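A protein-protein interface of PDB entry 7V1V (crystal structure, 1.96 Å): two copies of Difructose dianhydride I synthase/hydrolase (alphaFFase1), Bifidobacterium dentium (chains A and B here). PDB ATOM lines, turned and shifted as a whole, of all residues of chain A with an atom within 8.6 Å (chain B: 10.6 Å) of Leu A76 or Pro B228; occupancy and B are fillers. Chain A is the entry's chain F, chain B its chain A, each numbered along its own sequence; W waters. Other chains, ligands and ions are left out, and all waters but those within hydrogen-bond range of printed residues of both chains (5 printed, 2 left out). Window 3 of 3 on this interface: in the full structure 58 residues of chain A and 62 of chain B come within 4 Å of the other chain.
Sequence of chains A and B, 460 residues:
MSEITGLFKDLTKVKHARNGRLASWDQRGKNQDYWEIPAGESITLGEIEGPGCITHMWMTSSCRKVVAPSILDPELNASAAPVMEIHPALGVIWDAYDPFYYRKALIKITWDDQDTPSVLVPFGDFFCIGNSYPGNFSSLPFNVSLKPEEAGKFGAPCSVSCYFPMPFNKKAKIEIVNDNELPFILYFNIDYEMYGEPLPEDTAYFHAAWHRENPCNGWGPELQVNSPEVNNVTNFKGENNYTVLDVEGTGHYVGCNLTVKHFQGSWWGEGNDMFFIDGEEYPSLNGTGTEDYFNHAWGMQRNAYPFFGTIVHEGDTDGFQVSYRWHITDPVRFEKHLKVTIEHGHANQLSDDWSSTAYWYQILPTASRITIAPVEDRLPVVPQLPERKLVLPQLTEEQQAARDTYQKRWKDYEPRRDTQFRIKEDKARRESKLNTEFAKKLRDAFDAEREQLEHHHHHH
O of Ser A79 lies within hydrogen-bond range of ND2 of Asn B231. The side-chain amide nitrogen (ND2) of Asn B231 is in hydrogen-bond range of the backbone carbonyl oxygen (O) of Ala A80. The side-chain amide oxygen (OD1) of Asn B231 sits at hydrogen-bond distance from the side-chain amide nitrogen (ND2) of Asn A31, 3.0 Å away. The side-chain amide oxygen (OD1) of Asn B232 is in hydrogen-bond range of the side-chain hydroxyl (OG) of Ser A79, at 3.0 Å. The side-chain amide nitrogen (ND2) of Asn B226 sits close to the side-chain amide nitrogen (ND2) of Asn A31 (3.3 Å).
A ring nitrogen (NE2) of His B346 is in hydrogen-bond range of the backbone carbonyl oxygen of Val B233, 2.6 Å away. N of Leu A76 lies within hydrogen-bond range of OD1 of Asp A73, at 2.9 Å. The side-chain amide nitrogen (ND2) of Asn B226 is in hydrogen-bond range of the side-chain amide oxygen (OD1) of Asn B231 (3.3 Å). The backbone carbonyl oxygen (O) of Pro B228 sits close to the side-chain amide oxygen (OD1) of Asn B232 (3.5 Å).
CB of Lys A30 touches O of Asn B231 (3.3 Å). Lys A30 touches Asn B232. Val B233 touches Lys A30. Thr B234 touches Lys A30 (CG2 to CE, 3.8 Å). His B346 touches Lys A30 (CE1 to C, 3.2 Å). His B346 touches Asn A31 (CE1 to N, 3.5 Å). O of Leu A76 touches CG of Pro B228, at 3.6 Å. Pro B228 touches Ser A79 (CA to O, 3.8 Å). Ala A80 touches Asn B226. Ala A81 touches Asn B226.
Gln A32 touches none of the printed residues of chain B. No residue of chain B comes within 4 Å of Asp A73. No residue of chain B comes within 4 Å of Pro A74. Printed residues of chain B within 4 Å of Leu A76: Pro B228. No residue of chain B comes within 4 Å of Asn A77. No residue of chain B comes within 4 Å of Ala A78. Ser A79 touches just these residues of chain B: Pro B228 (3.8 Å), Asn B231 (2.7 Å) and Asn B232 (3.0 Å). Ala A80 touches two residues of chain B. Printed residues of chain B within 4 Å of Ala A81: Asn B226. Met A84 touches none of the printed residues of chain B. Pro B228 touches two residues of chain A. Printed residues of chain A within 4 Å of Asn B231: Lys A30 (3.3 Å), Asn A31 (3.0 Å), Ser A79 (2.7 Å) and Ala A80 (3.4 Å). Of the printed residues of chain A, Asn B232 touches Lys A30 (3.5 Å) and Ser A79 (3.0 Å). The nearest residue of chain B that does not touch Leu A76 is Glu B229 (6.1 Å). The nearest residue of chain A that does not touch Pro B228 is Ala A80 (4.5 Å). The nearest printed residue of chain B that does not touch Lys A30 is Val B230 (6.5 Å).
Of the 17 printed residues of chain A, 6 touch a printed residue of chain B. Hydrophobic or aromatic side chains of chain A within 4 Å of the printed part of chain B: Ala A80. Along chain A the printed residues that touch a printed residue of chain B span positions 30 to 81. Of the 16 printed residues of chain B, 7 touch a printed residue of chain A. Printed residues of chain B that touch a printed residue of chain A: Asn B226, Pro B228, Asn B231, Asn B232, Val B233, Thr B234 and His B346. Hydrophobic or aromatic side chains of chain B within 4 Å of the printed part of chain A: Pro B228 and His B346. Among the printed residues, no Asp or Glu carboxylate lies within 4 Å of a Lys or Arg side-chain nitrogen of the other chain.
No position is printed for both chains. Of the 15 pairs that touch across the chains among the printed residues, none has its exchanged pair printed and touching as well.
Water W4 lies within hydrogen-bond range of the side-chain amide nitrogen (ND2) of Asn B232 (2.7 Å) and the side-chain amide nitrogen (NE2) of Gln A32 (3.1 Å). Water W3 lies within hydrogen-bond range of O of Asn A31, O of Ala A80 and ND2 of Asn B231. Water W5 lies within hydrogen-bond range of ND2 of Asn B226 (2.8 Å), OD1 of Asn B231 (2.8 Å) and ND2 of Asn A31 (3.5 Å). Water W1 bridges the backbone carbonyl oxygen of Ser A79 (2.8 Å) and the side-chain amide nitrogen of Asn B231 (3.3 Å). Water W2 lies within hydrogen-bond range of ND2 of Asn B232 (3.0 Å), OG of Ser A79 (3.1 Å) and NE2 of Gln A32 (3.5 Å).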
ATOM      1  N   LYS A  30     -10.368  12.451  13.051  1.00  0.00           N
ATOM      2  CA  LYS A  30     -10.687  12.934  14.414  1.00  0.00           C
ATOM      3  C   LYS A  30     -12.146  13.389  14.422  1.00  0.00           C
ATOM      4  O   LYS A  30     -12.873  12.984  13.501  1.00  0.00           O
ATOM      5  CB  LYS A  30      -9.678  14.022  14.789  1.00  0.00           C
ATOM      6  CG  LYS A  30      -8.244  13.520  14.843  1.00  0.00           C
ATOM      7  CD  LYS A  30      -7.209  14.585  15.116  1.00  0.00           C
ATOM      8  CE  LYS A  30      -5.810  14.007  15.095  1.00  0.00           C
ATOM      9  NZ  LYS A  30      -4.888  14.858  15.880  1.00  0.00           N
ATOM     10  N   ASN A  31     -12.572  14.194  15.403  1.00  0.00           N
ATOM     11  CA  ASN A  31     -14.027  14.463  15.596  1.00  0.00           C
ATOM     12  C   ASN A  31     -14.407  15.899  15.228  1.00  0.00           C
ATOM     13  O   ASN A  31     -15.413  16.422  15.817  1.00  0.00           O
ATOM     14  CB  ASN A  31     -14.489  14.149  17.016  1.00  0.00           C
ATOM     15  CG  ASN A  31     -16.002  13.972  17.076  1.00  0.00           C
ATOM     16  OD1 ASN A  31     -16.629  13.505  16.111  1.00  0.00           O
ATOM     17  ND2 ASN A  31     -16.593  14.420  18.174  1.00  0.00           N
ATOM     18  N   GLN A  32     -13.694  16.511  14.278  1.00  0.00           N
ATOM     19  CA  GLN A  32     -14.123  17.807  13.683  1.00  0.00           C
ATOM     20  C   GLN A  32     -14.718  17.510  12.305  1.00  0.00           C
ATOM     21  O   GLN A  32     -14.082  17.881  11.272  1.00  0.00           O
ATOM     22  CB  GLN A  32     -12.997  18.831  13.575  1.00  0.00           C
ATOM     23  CG  GLN A  32     -12.490  19.355  14.901  1.00  0.00           C
ATOM     24  CD  GLN A  32     -11.456  20.447  14.701  1.00  0.00           C
ATOM     25  OE1 GLN A  32     -11.434  21.180  13.696  1.00  0.00           O
ATOM     26  NE2 GLN A  32     -10.630  20.611  15.722  1.00  0.00           N
ATOM     27  N   LEU A  72     -12.462  29.690  29.584  1.00  0.00           N
ATOM     28  CA  LEU A  72     -12.143  28.399  28.913  1.00  0.00           C
ATOM     29  C   LEU A  72     -10.837  28.603  28.134  1.00  0.00           C
ATOM     30  O   LEU A  72     -10.822  29.447  27.260  1.00  0.00           O
ATOM     31  CB  LEU A  72     -13.272  27.965  27.969  1.00  0.00           C
ATOM     32  CG  LEU A  72     -14.473  27.300  28.633  1.00  0.00           C
ATOM     33  CD1 LEU A  72     -15.441  28.343  29.211  1.00  0.00           C
ATOM     34  CD2 LEU A  72     -15.194  26.411  27.644  1.00  0.00           C
ATOM     35  N   ASP A  73      -9.815  27.813  28.427  1.00  0.00           N
ATOM     36  CA  ASP A  73      -8.543  27.785  27.654  1.00  0.00           C
ATOM     37  C   ASP A  73      -8.874  27.682  26.173  1.00  0.00           C
ATOM     38  O   ASP A  73      -9.487  26.708  25.758  1.00  0.00           O
ATOM     39  CB  ASP A  73      -7.674  26.609  28.066  1.00  0.00           C
ATOM     40  CG  ASP A  73      -6.397  26.572  27.249  1.00  0.00           C
ATOM     41  OD1 ASP A  73      -6.439  26.099  26.128  1.00  0.00           O
ATOM     42  OD2 ASP A  73      -5.401  27.088  27.724  1.00  0.00           O
ATOM     43  N   PRO A  74      -8.586  28.705  25.343  1.00  0.00           N
ATOM     44  CA  PRO A  74      -9.068  28.709  23.955  1.00  0.00           C
ATOM     45  C   PRO A  74      -8.428  27.672  23.015  1.00  0.00           C
ATOM     46  O   PRO A  74      -9.073  27.258  22.023  1.00  0.00           O
ATOM     47  CB  PRO A  74      -8.820  30.154  23.477  1.00  0.00           C
ATOM     48  CG  PRO A  74      -7.817  30.740  24.454  1.00  0.00           C
ATOM     49  CD  PRO A  74      -8.008  29.986  25.758  1.00  0.00           C
ATOM     50  N   GLU A  75      -7.199  27.251  23.303  1.00  0.00           N
ATOM     51  CA  GLU A  75      -6.521  26.226  22.469  1.00  0.00           C
ATOM     52  C   GLU A  75      -7.204  24.868  22.713  1.00  0.00           C
ATOM     53  O   GLU A  75      -7.556  24.182  21.719  1.00  0.00           O
ATOM     54  CB  GLU A  75      -5.013  26.242  22.734  1.00  0.00           C
ATOM     55  CG  GLU A  75      -4.324  27.532  22.251  1.00  0.00           C
ATOM     56  CD  GLU A  75      -4.512  28.808  23.076  1.00  0.00           C
ATOM     57  OE1 GLU A  75      -4.653  28.705  24.330  1.00  0.00           O
ATOM     58  OE2 GLU A  75      -4.529  29.916  22.461  1.00  0.00           O
ATOM     59  N   LEU A  76      -7.387  24.479  23.972  1.00  0.00           N
ATOM     60  CA  LEU A  76      -8.074  23.204  24.314  1.00  0.00           C
ATOM     61  C   LEU A  76      -9.541  23.300  23.882  1.00  0.00           C
ATOM     62  O   LEU A  76     -10.057  22.289  23.418  1.00  0.00           O
ATOM     63  CB  LEU A  76      -7.966  22.915  25.809  1.00  0.00           C
ATOM     64  CG  LEU A  76      -6.583  22.547  26.338  1.00  0.00           C
ATOM     65  CD1 LEU A  76      -6.614  22.415  27.862  1.00  0.00           C
ATOM     66  CD2 LEU A  76      -6.086  21.258  25.694  1.00  0.00           C
ATOM     67  N   ASN A  77     -10.171  24.480  24.009  1.00  0.00           N
ATOM     68  CA  ASN A  77     -11.610  24.689  23.701  1.00  0.00           C
ATOM     69  C   ASN A  77     -11.840  24.343  22.220  1.00  0.00           C
ATOM     70  O   ASN A  77     -12.908  23.785  21.902  1.00  0.00           O
ATOM     71  CB  ASN A  77     -12.071  26.098  24.084  1.00  0.00           C
ATOM     72  CG  ASN A  77     -13.577  26.281  24.191  1.00  0.00           C
ATOM     73  OD1 ASN A  77     -14.380  25.360  23.977  1.00  0.00           O
ATOM     74  ND2 ASN A  77     -13.971  27.491  24.531  1.00  0.00           N
ATOM     75  N   ALA A  78     -10.847  24.586  21.350  1.00  0.00           N
ATOM     76  CA  ALA A  78     -10.948  24.329  19.895  1.00  0.00           C
ATOM     77  C   ALA A  78     -11.270  22.852  19.609  1.00  0.00           C
ATOM     78  O   ALA A  78     -11.915  22.594  18.583  1.00  0.00           O
ATOM     79  CB  ALA A  78      -9.672  24.736  19.210  1.00  0.00           C
ATOM     80  N   SER A  79     -10.766  21.937  20.438  1.00  0.00           N
ATOM     81  CA  SER A  79     -10.874  20.462  20.281  1.00  0.00           C
ATOM     82  C   SER A  79     -12.051  19.875  21.075  1.00  0.00           C
ATOM     83  O   SER A  79     -12.283  18.660  20.943  1.00  0.00           O
ATOM     84  CB  SER A  79      -9.583  19.801  20.701  1.00  0.00           C
ATOM     85  OG  SER A  79      -8.672  19.905  19.631  1.00  0.00           O
ATOM     86  N   ALA A  80     -12.758  20.674  21.875  1.00  0.00           N
ATOM     87  CA  ALA A  80     -13.995  20.228  22.552  1.00  0.00           C
ATOM     88  C   ALA A  80     -15.127  20.236  21.524  1.00  0.00           C
ATOM     89  O   ALA A  80     -14.835  20.236  20.304  1.00  0.00           O
ATOM     90  CB  ALA A  80     -14.304  21.082  23.761  1.00  0.00           C
ATOM     91  N   ALA A  81     -16.379  20.257  21.985  1.00  0.00           N
ATOM     92  CA  ALA A  81     -17.563  20.381  21.111  1.00  0.00           C
ATOM     93  C   ALA A  81     -17.388  21.668  20.302  1.00  0.00           C
ATOM     94  O   ALA A  81     -16.770  22.609  20.772  1.00  0.00           O
ATOM     95  CB  ALA A  81     -18.831  20.392  21.920  1.00  0.00           C
ATOM     96  N   MET A  84     -20.101  26.450  21.756  1.00  0.00           N
ATOM     97  CA  MET A  84     -20.222  26.601  23.230  1.00  0.00           C
ATOM     98  C   MET A  84     -21.627  27.126  23.567  1.00  0.00           C
ATOM     99  O   MET A  84     -21.810  28.353  23.719  1.00  0.00           O
ATOM    100  CB  MET A  84     -19.115  27.501  23.767  1.00  0.00           C
ATOM    101  CG  MET A  84     -17.747  26.817  23.711  1.00  0.00           C
ATOM    102  SD  MET A  84     -17.659  25.338  24.771  1.00  0.00           S
ATOM    103  CE  MET A  84     -17.805  23.995  23.599  1.00  0.00           C
ATOM    104  N   ARG A 416      -6.373  34.885  20.496  1.00  0.00           N
ATOM    105  CA  ARG A 416      -6.201  33.426  20.698  1.00  0.00           C
ATOM    106  C   ARG A 416      -7.391  32.703  20.064  1.00  0.00           C
ATOM    107  O   ARG A 416      -7.181  31.598  19.514  1.00  0.00           O
ATOM    108  CB  ARG A 416      -6.000  33.116  22.178  1.00  0.00           C
ATOM    109  CG  ARG A 416      -4.723  33.734  22.739  1.00  0.00           C
ATOM    110  CD  ARG A 416      -4.653  33.703  24.248  1.00  0.00           C
ATOM    111  NE  ARG A 416      -4.600  32.320  24.687  1.00  0.00           N
ATOM    112  CZ  ARG A 416      -4.534  31.921  25.951  1.00  0.00           C
ATOM    113  NH1 ARG A 416      -4.494  32.810  26.928  1.00  0.00           N
ATOM    114  NH2 ARG A 416      -4.484  30.631  26.231  1.00  0.00           N
ATOM    115  N   GLN A 420      -7.554  30.143  16.338  1.00  0.00           N
ATOM    116  CA  GLN A 420      -8.254  28.837  16.266  1.00  0.00           C
ATOM    117  C   GLN A 420      -9.245  28.818  15.098  1.00  0.00           C
ATOM    118  O   GLN A 420      -9.366  27.748  14.482  1.00  0.00           O
ATOM    119  CB  GLN A 420      -8.931  28.488  17.599  1.00  0.00           C
ATOM    120  CG  GLN A 420      -7.956  28.190  18.724  1.00  0.00           C
ATOM    121  CD  GLN A 420      -6.816  27.271  18.345  1.00  0.00           C
ATOM    122  OE1 GLN A 420      -7.002  26.196  17.795  1.00  0.00           O
ATOM    123  NE2 GLN A 420      -5.595  27.692  18.643  1.00  0.00           N
ATOM    124  N   LYS A 424      -8.932  26.206  11.695  1.00  0.00           N
ATOM    125  CA  LYS A 424     -10.077  25.395  11.199  1.00  0.00           C
ATOM    126  C   LYS A 424     -10.344  25.764   9.751  1.00  0.00           C
ATOM    127  O   LYS A 424     -10.644  24.843   9.000  1.00  0.00           O
ATOM    128  CB  LYS A 424     -11.313  25.538  12.083  1.00  0.00           C
ATOM    129  CG  LYS A 424     -11.111  24.925  13.445  1.00  0.00           C
ATOM    130  CD  LYS A 424     -12.228  25.114  14.431  1.00  0.00           C
ATOM    131  CE  LYS A 424     -12.055  24.190  15.615  1.00  0.00           C
ATOM    132  NZ  LYS A 424     -12.944  24.511  16.767  1.00  0.00           N
ATOM    133  N   TRP B 219     -13.094   2.205  24.170  1.00  0.00           N
ATOM    134  CA  TRP B 219     -11.694   2.354  24.678  1.00  0.00           C
ATOM    135  C   TRP B 219     -11.635   3.383  25.809  1.00  0.00           C
ATOM    136  O   TRP B 219     -10.609   3.392  26.553  1.00  0.00           O
ATOM    137  CB  TRP B 219     -10.720   2.703  23.553  1.00  0.00           C
ATOM    138  CG  TRP B 219     -11.014   3.980  22.833  1.00  0.00           C
ATOM    139  CD1 TRP B 219     -11.615   4.114  21.615  1.00  0.00           C
ATOM    140  CD2 TRP B 219     -10.718   5.312  23.286  1.00  0.00           C
ATOM    141  NE1 TRP B 219     -11.708   5.438  21.279  1.00  0.00           N
ATOM    142  CE2 TRP B 219     -11.171   6.194  22.288  1.00  0.00           C
ATOM    143  CE3 TRP B 219     -10.108   5.845  24.427  1.00  0.00           C
ATOM    144  CZ2 TRP B 219     -11.038   7.574  22.405  1.00  0.00           C
ATOM    145  CZ3 TRP B 219      -9.946   7.212  24.531  1.00  0.00           C
ATOM    146  CH2 TRP B 219     -10.404   8.062  23.530  1.00  0.00           C
ATOM    147  N   LEU B 223     -14.132   8.366  30.027  1.00  0.00           N
ATOM    148  CA  LEU B 223     -13.678   9.734  29.667  1.00  0.00           C
ATOM    149  C   LEU B 223     -14.917  10.497  29.228  1.00  0.00           C
ATOM    150  O   LEU B 223     -15.770   9.898  28.563  1.00  0.00           O
ATOM    151  CB  LEU B 223     -12.661   9.760  28.522  1.00  0.00           C
ATOM    152  CG  LEU B 223     -11.224   9.374  28.857  1.00  0.00           C
ATOM    153  CD1 LEU B 223     -11.117   7.904  29.218  1.00  0.00           C
ATOM    154  CD2 LEU B 223     -10.318   9.692  27.679  1.00  0.00           C
ATOM    155  N   GLN B 224     -14.963  11.782  29.548  1.00  0.00           N
ATOM    156  CA  GLN B 224     -16.061  12.667  29.125  1.00  0.00           C
ATOM    157  C   GLN B 224     -16.088  12.740  27.595  1.00  0.00           C
ATOM    158  O   GLN B 224     -15.023  13.090  26.959  1.00  0.00           O
ATOM    159  CB  GLN B 224     -15.877  14.070  29.703  1.00  0.00           C
ATOM    160  CG  GLN B 224     -16.959  15.033  29.225  1.00  0.00           C
ATOM    161  CD  GLN B 224     -16.972  16.271  30.085  1.00  0.00           C
ATOM    162  OE1 GLN B 224     -16.107  16.474  30.944  1.00  0.00           O
ATOM    163  NE2 GLN B 224     -17.975  17.092  29.881  1.00  0.00           N
ATOM    164  N   VAL B 225     -17.271  12.491  27.025  1.00  0.00           N
ATOM    165  CA  VAL B 225     -17.559  12.718  25.582  1.00  0.00           C
ATOM    166  C   VAL B 225     -17.209  14.172  25.241  1.00  0.00           C
ATOM    167  O   VAL B 225     -17.458  15.088  26.048  1.00  0.00           O
ATOM    168  CB  VAL B 225     -19.007  12.352  25.204  1.00  0.00           C
ATOM    169  CG1 VAL B 225     -19.357  12.801  23.783  1.00  0.00           C
ATOM    170  CG2 VAL B 225     -19.235  10.862  25.362  1.00  0.00           C
ATOM    171  N   ASN B 226     -16.557  14.329  24.103  1.00  0.00           N
ATOM    172  CA  ASN B 226     -16.206  15.634  23.488  1.00  0.00           C
ATOM    173  C   ASN B 226     -15.103  16.336  24.290  1.00  0.00           C
ATOM    174  O   ASN B 226     -14.810  17.498  23.979  1.00  0.00           O
ATOM    175  CB  ASN B 226     -17.453  16.496  23.293  1.00  0.00           C
ATOM    176  CG  ASN B 226     -18.268  16.069  22.095  1.00  0.00           C
ATOM    177  OD1 ASN B 226     -19.485  16.291  22.055  1.00  0.00           O
ATOM    178  ND2 ASN B 226     -17.624  15.527  21.080  1.00  0.00           N
ATOM    179  N   SER B 227     -14.466  15.659  25.230  1.00  0.00           N
ATOM    180  CA  SER B 227     -13.192  16.143  25.821  1.00  0.00           C
ATOM    181  C   SER B 227     -12.149  16.227  24.702  1.00  0.00           C
ATOM    182  O   SER B 227     -12.218  15.504  23.704  1.00  0.00           O
ATOM    183  CB  SER B 227     -12.723  15.297  26.968  1.00  0.00           C
ATOM    184  OG  SER B 227     -12.449  13.978  26.531  1.00  0.00           O
ATOM    185  N   PRO B 228     -11.196  17.176  24.786  1.00  0.00           N
ATOM    186  CA  PRO B 228     -10.131  17.275  23.782  1.00  0.00           C
ATOM    187  C   PRO B 228      -9.401  15.930  23.572  1.00  0.00           C
ATOM    188  O   PRO B 228      -9.109  15.606  22.474  1.00  0.00           O
ATOM    189  CB  PRO B 228      -9.208  18.347  24.370  1.00  0.00           C
ATOM    190  CG  PRO B 228     -10.129  19.198  25.217  1.00  0.00           C
ATOM    191  CD  PRO B 228     -11.101  18.219  25.828  1.00  0.00           C
ATOM    192  N   GLU B 229      -9.193  15.152  24.625  1.00  0.00           N
ATOM    193  CA  GLU B 229      -8.472  13.850  24.534  1.00  0.00           C
ATOM    194  C   GLU B 229      -9.256  12.879  23.645  1.00  0.00           C
ATOM    195  O   GLU B 229      -8.656  12.237  22.755  1.00  0.00           O
ATOM    196  CB  GLU B 229      -8.232  13.266  25.923  1.00  0.00           C
ATOM    197  CG  GLU B 229      -7.263  14.077  26.757  1.00  0.00           C
ATOM    198  CD  GLU B 229      -7.888  15.243  27.530  1.00  0.00           C
ATOM    199  OE1 GLU B 229      -9.100  15.561  27.310  1.00  0.00           O
ATOM    200  OE2 GLU B 229      -7.154  15.867  28.330  1.00  0.00           O
ATOM    201  N   VAL B 230     -10.556  12.756  23.889  1.00  0.00           N
ATOM    202  CA  VAL B 230     -11.424  11.875  23.075  1.00  0.00           C
ATOM    203  C   VAL B 230     -11.395  12.383  21.636  1.00  0.00           C
ATOM    204  O   VAL B 230     -11.167  11.560  20.732  1.00  0.00           O
ATOM    205  CB  VAL B 230     -12.846  11.789  23.653  1.00  0.00           C
ATOM    206  CG1 VAL B 230     -13.839  11.254  22.618  1.00  0.00           C
ATOM    207  CG2 VAL B 230     -12.855  10.972  24.931  1.00  0.00           C
ATOM    208  N   ASN B 231     -11.595  13.684  21.417  1.00  0.00           N
ATOM    209  CA  ASN B 231     -11.837  14.217  20.049  1.00  0.00           C
ATOM    210  C   ASN B 231     -10.589  14.098  19.159  1.00  0.00           C
ATOM    211  O   ASN B 231     -10.770  14.116  17.941  1.00  0.00           O
ATOM    212  CB  ASN B 231     -12.357  15.645  20.088  1.00  0.00           C
ATOM    213  CG  ASN B 231     -13.845  15.716  20.387  1.00  0.00           C
ATOM    214  OD1 ASN B 231     -14.548  14.711  20.332  1.00  0.00           O
ATOM    215  ND2 ASN B 231     -14.330  16.907  20.692  1.00  0.00           N
ATOM    216  N   ASN B 232      -9.385  13.955  19.726  1.00  0.00           N
ATOM    217  CA  ASN B 232      -8.119  13.959  18.950  1.00  0.00           C
ATOM    218  C   ASN B 232      -7.660  12.503  18.686  1.00  0.00           C
ATOM    219  O   ASN B 232      -6.606  12.314  18.064  1.00  0.00           O
ATOM    220  CB  ASN B 232      -7.129  14.949  19.590  1.00  0.00           C
ATOM    221  CG  ASN B 232      -7.485  16.398  19.260  1.00  0.00           C
ATOM    222  OD1 ASN B 232      -7.309  17.309  20.065  1.00  0.00           O
ATOM    223  ND2 ASN B 232      -8.055  16.639  18.095  1.00  0.00           N
ATOM    224  N   VAL B 233      -8.470  11.509  19.032  1.00  0.00           N
ATOM    225  CA  VAL B 233      -8.249  10.089  18.624  1.00  0.00           C
ATOM    226  C   VAL B 233      -8.712   9.946  17.168  1.00  0.00           C
ATOM    227  O   VAL B 233      -9.729  10.559  16.757  1.00  0.00           O
ATOM    228  CB  VAL B 233      -8.888   9.103  19.629  1.00  0.00           C
ATOM    229  CG1 VAL B 233      -8.830   7.644  19.222  1.00  0.00           C
ATOM    230  CG2 VAL B 233      -8.236   9.256  20.991  1.00  0.00           C
ATOM    231  N   THR B 234      -7.933   9.220  16.377  1.00  0.00           N
ATOM    232  CA  THR B 234      -8.182   9.018  14.931  1.00  0.00           C
ATOM    233  C   THR B 234      -8.859   7.672  14.740  1.00  0.00           C
ATOM    234  O   THR B 234      -8.553   6.744  15.501  1.00  0.00           O
ATOM    235  CB  THR B 234      -6.907   9.102  14.081  1.00  0.00           C
ATOM    236  OG1 THR B 234      -6.192   7.904  14.351  1.00  0.00           O
ATOM    237  CG2 THR B 234      -6.051  10.310  14.381  1.00  0.00           C
ATOM    238  N   HIS B 346     -17.401   8.825  19.108  1.00  0.00           N
ATOM    239  CA  HIS B 346     -16.235   9.126  18.249  1.00  0.00           C
ATOM    240  C   HIS B 346     -15.169   8.017  18.426  1.00  0.00           C
ATOM    241  O   HIS B 346     -14.857   7.659  19.562  1.00  0.00           O
ATOM    242  CB  HIS B 346     -15.616  10.476  18.584  1.00  0.00           C
ATOM    243  CG  HIS B 346     -14.323  10.661  17.876  1.00  0.00           C
ATOM    244  ND1 HIS B 346     -14.275  10.728  16.498  1.00  0.00           N
ATOM    245  CD2 HIS B 346     -13.047  10.703  18.326  1.00  0.00           C
ATOM    246  CE1 HIS B 346     -13.009  10.834  16.120  1.00  0.00           C
ATOM    247  NE2 HIS B 346     -12.227  10.856  17.231  1.00  0.00           N
ATOM    248  N   ALA B 347     -14.622   7.499  17.333  1.00  0.00           N
ATOM    249  CA  ALA B 347     -13.488   6.540  17.348  1.00  0.00           C
ATOM    250  C   ALA B 347     -13.825   5.389  18.294  1.00  0.00           C
ATOM    251  O   ALA B 347     -12.901   4.818  18.912  1.00  0.00           O
ATOM    252  CB  ALA B 347     -12.201   7.244  17.759  1.00  0.00           C
ATOM    253  N   GLN B 349     -15.218   5.246  21.195  1.00  0.00           N
ATOM    254  CA  GLN B 349     -14.951   5.622  22.606  1.00  0.00           C
ATOM    255  C   GLN B 349     -15.893   4.880  23.556  1.00  0.00           C
ATOM    256  O   GLN B 349     -15.470   4.439  24.678  1.00  0.00           O
ATOM    257  CB  GLN B 349     -15.193   7.130  22.765  1.00  0.00           C
ATOM    258  CG  GLN B 349     -14.977   7.610  24.190  1.00  0.00           C
ATOM    259  CD  GLN B 349     -15.821   8.784  24.613  1.00  0.00           C
ATOM    260  OE1 GLN B 349     -16.441   9.467  23.798  1.00  0.00           O
ATOM    261  NE2 GLN B 349     -15.825   9.029  25.916  1.00  0.00           N
HETATM  262  O   HOH W   1     -12.699  18.401  18.208  1.00  0.00           O
HETATM  263  O   HOH W   2      -7.606  19.248  16.790  1.00  0.00           O
HETATM  264  O   HOH W   3     -15.401  18.328  17.773  1.00  0.00           O
HETATM  265  O   HOH W   4     -10.284  17.790  17.027  1.00  0.00           O
HETATM  266  O   HOH W   5     -16.500  13.020  21.369  1.00  0.00           O
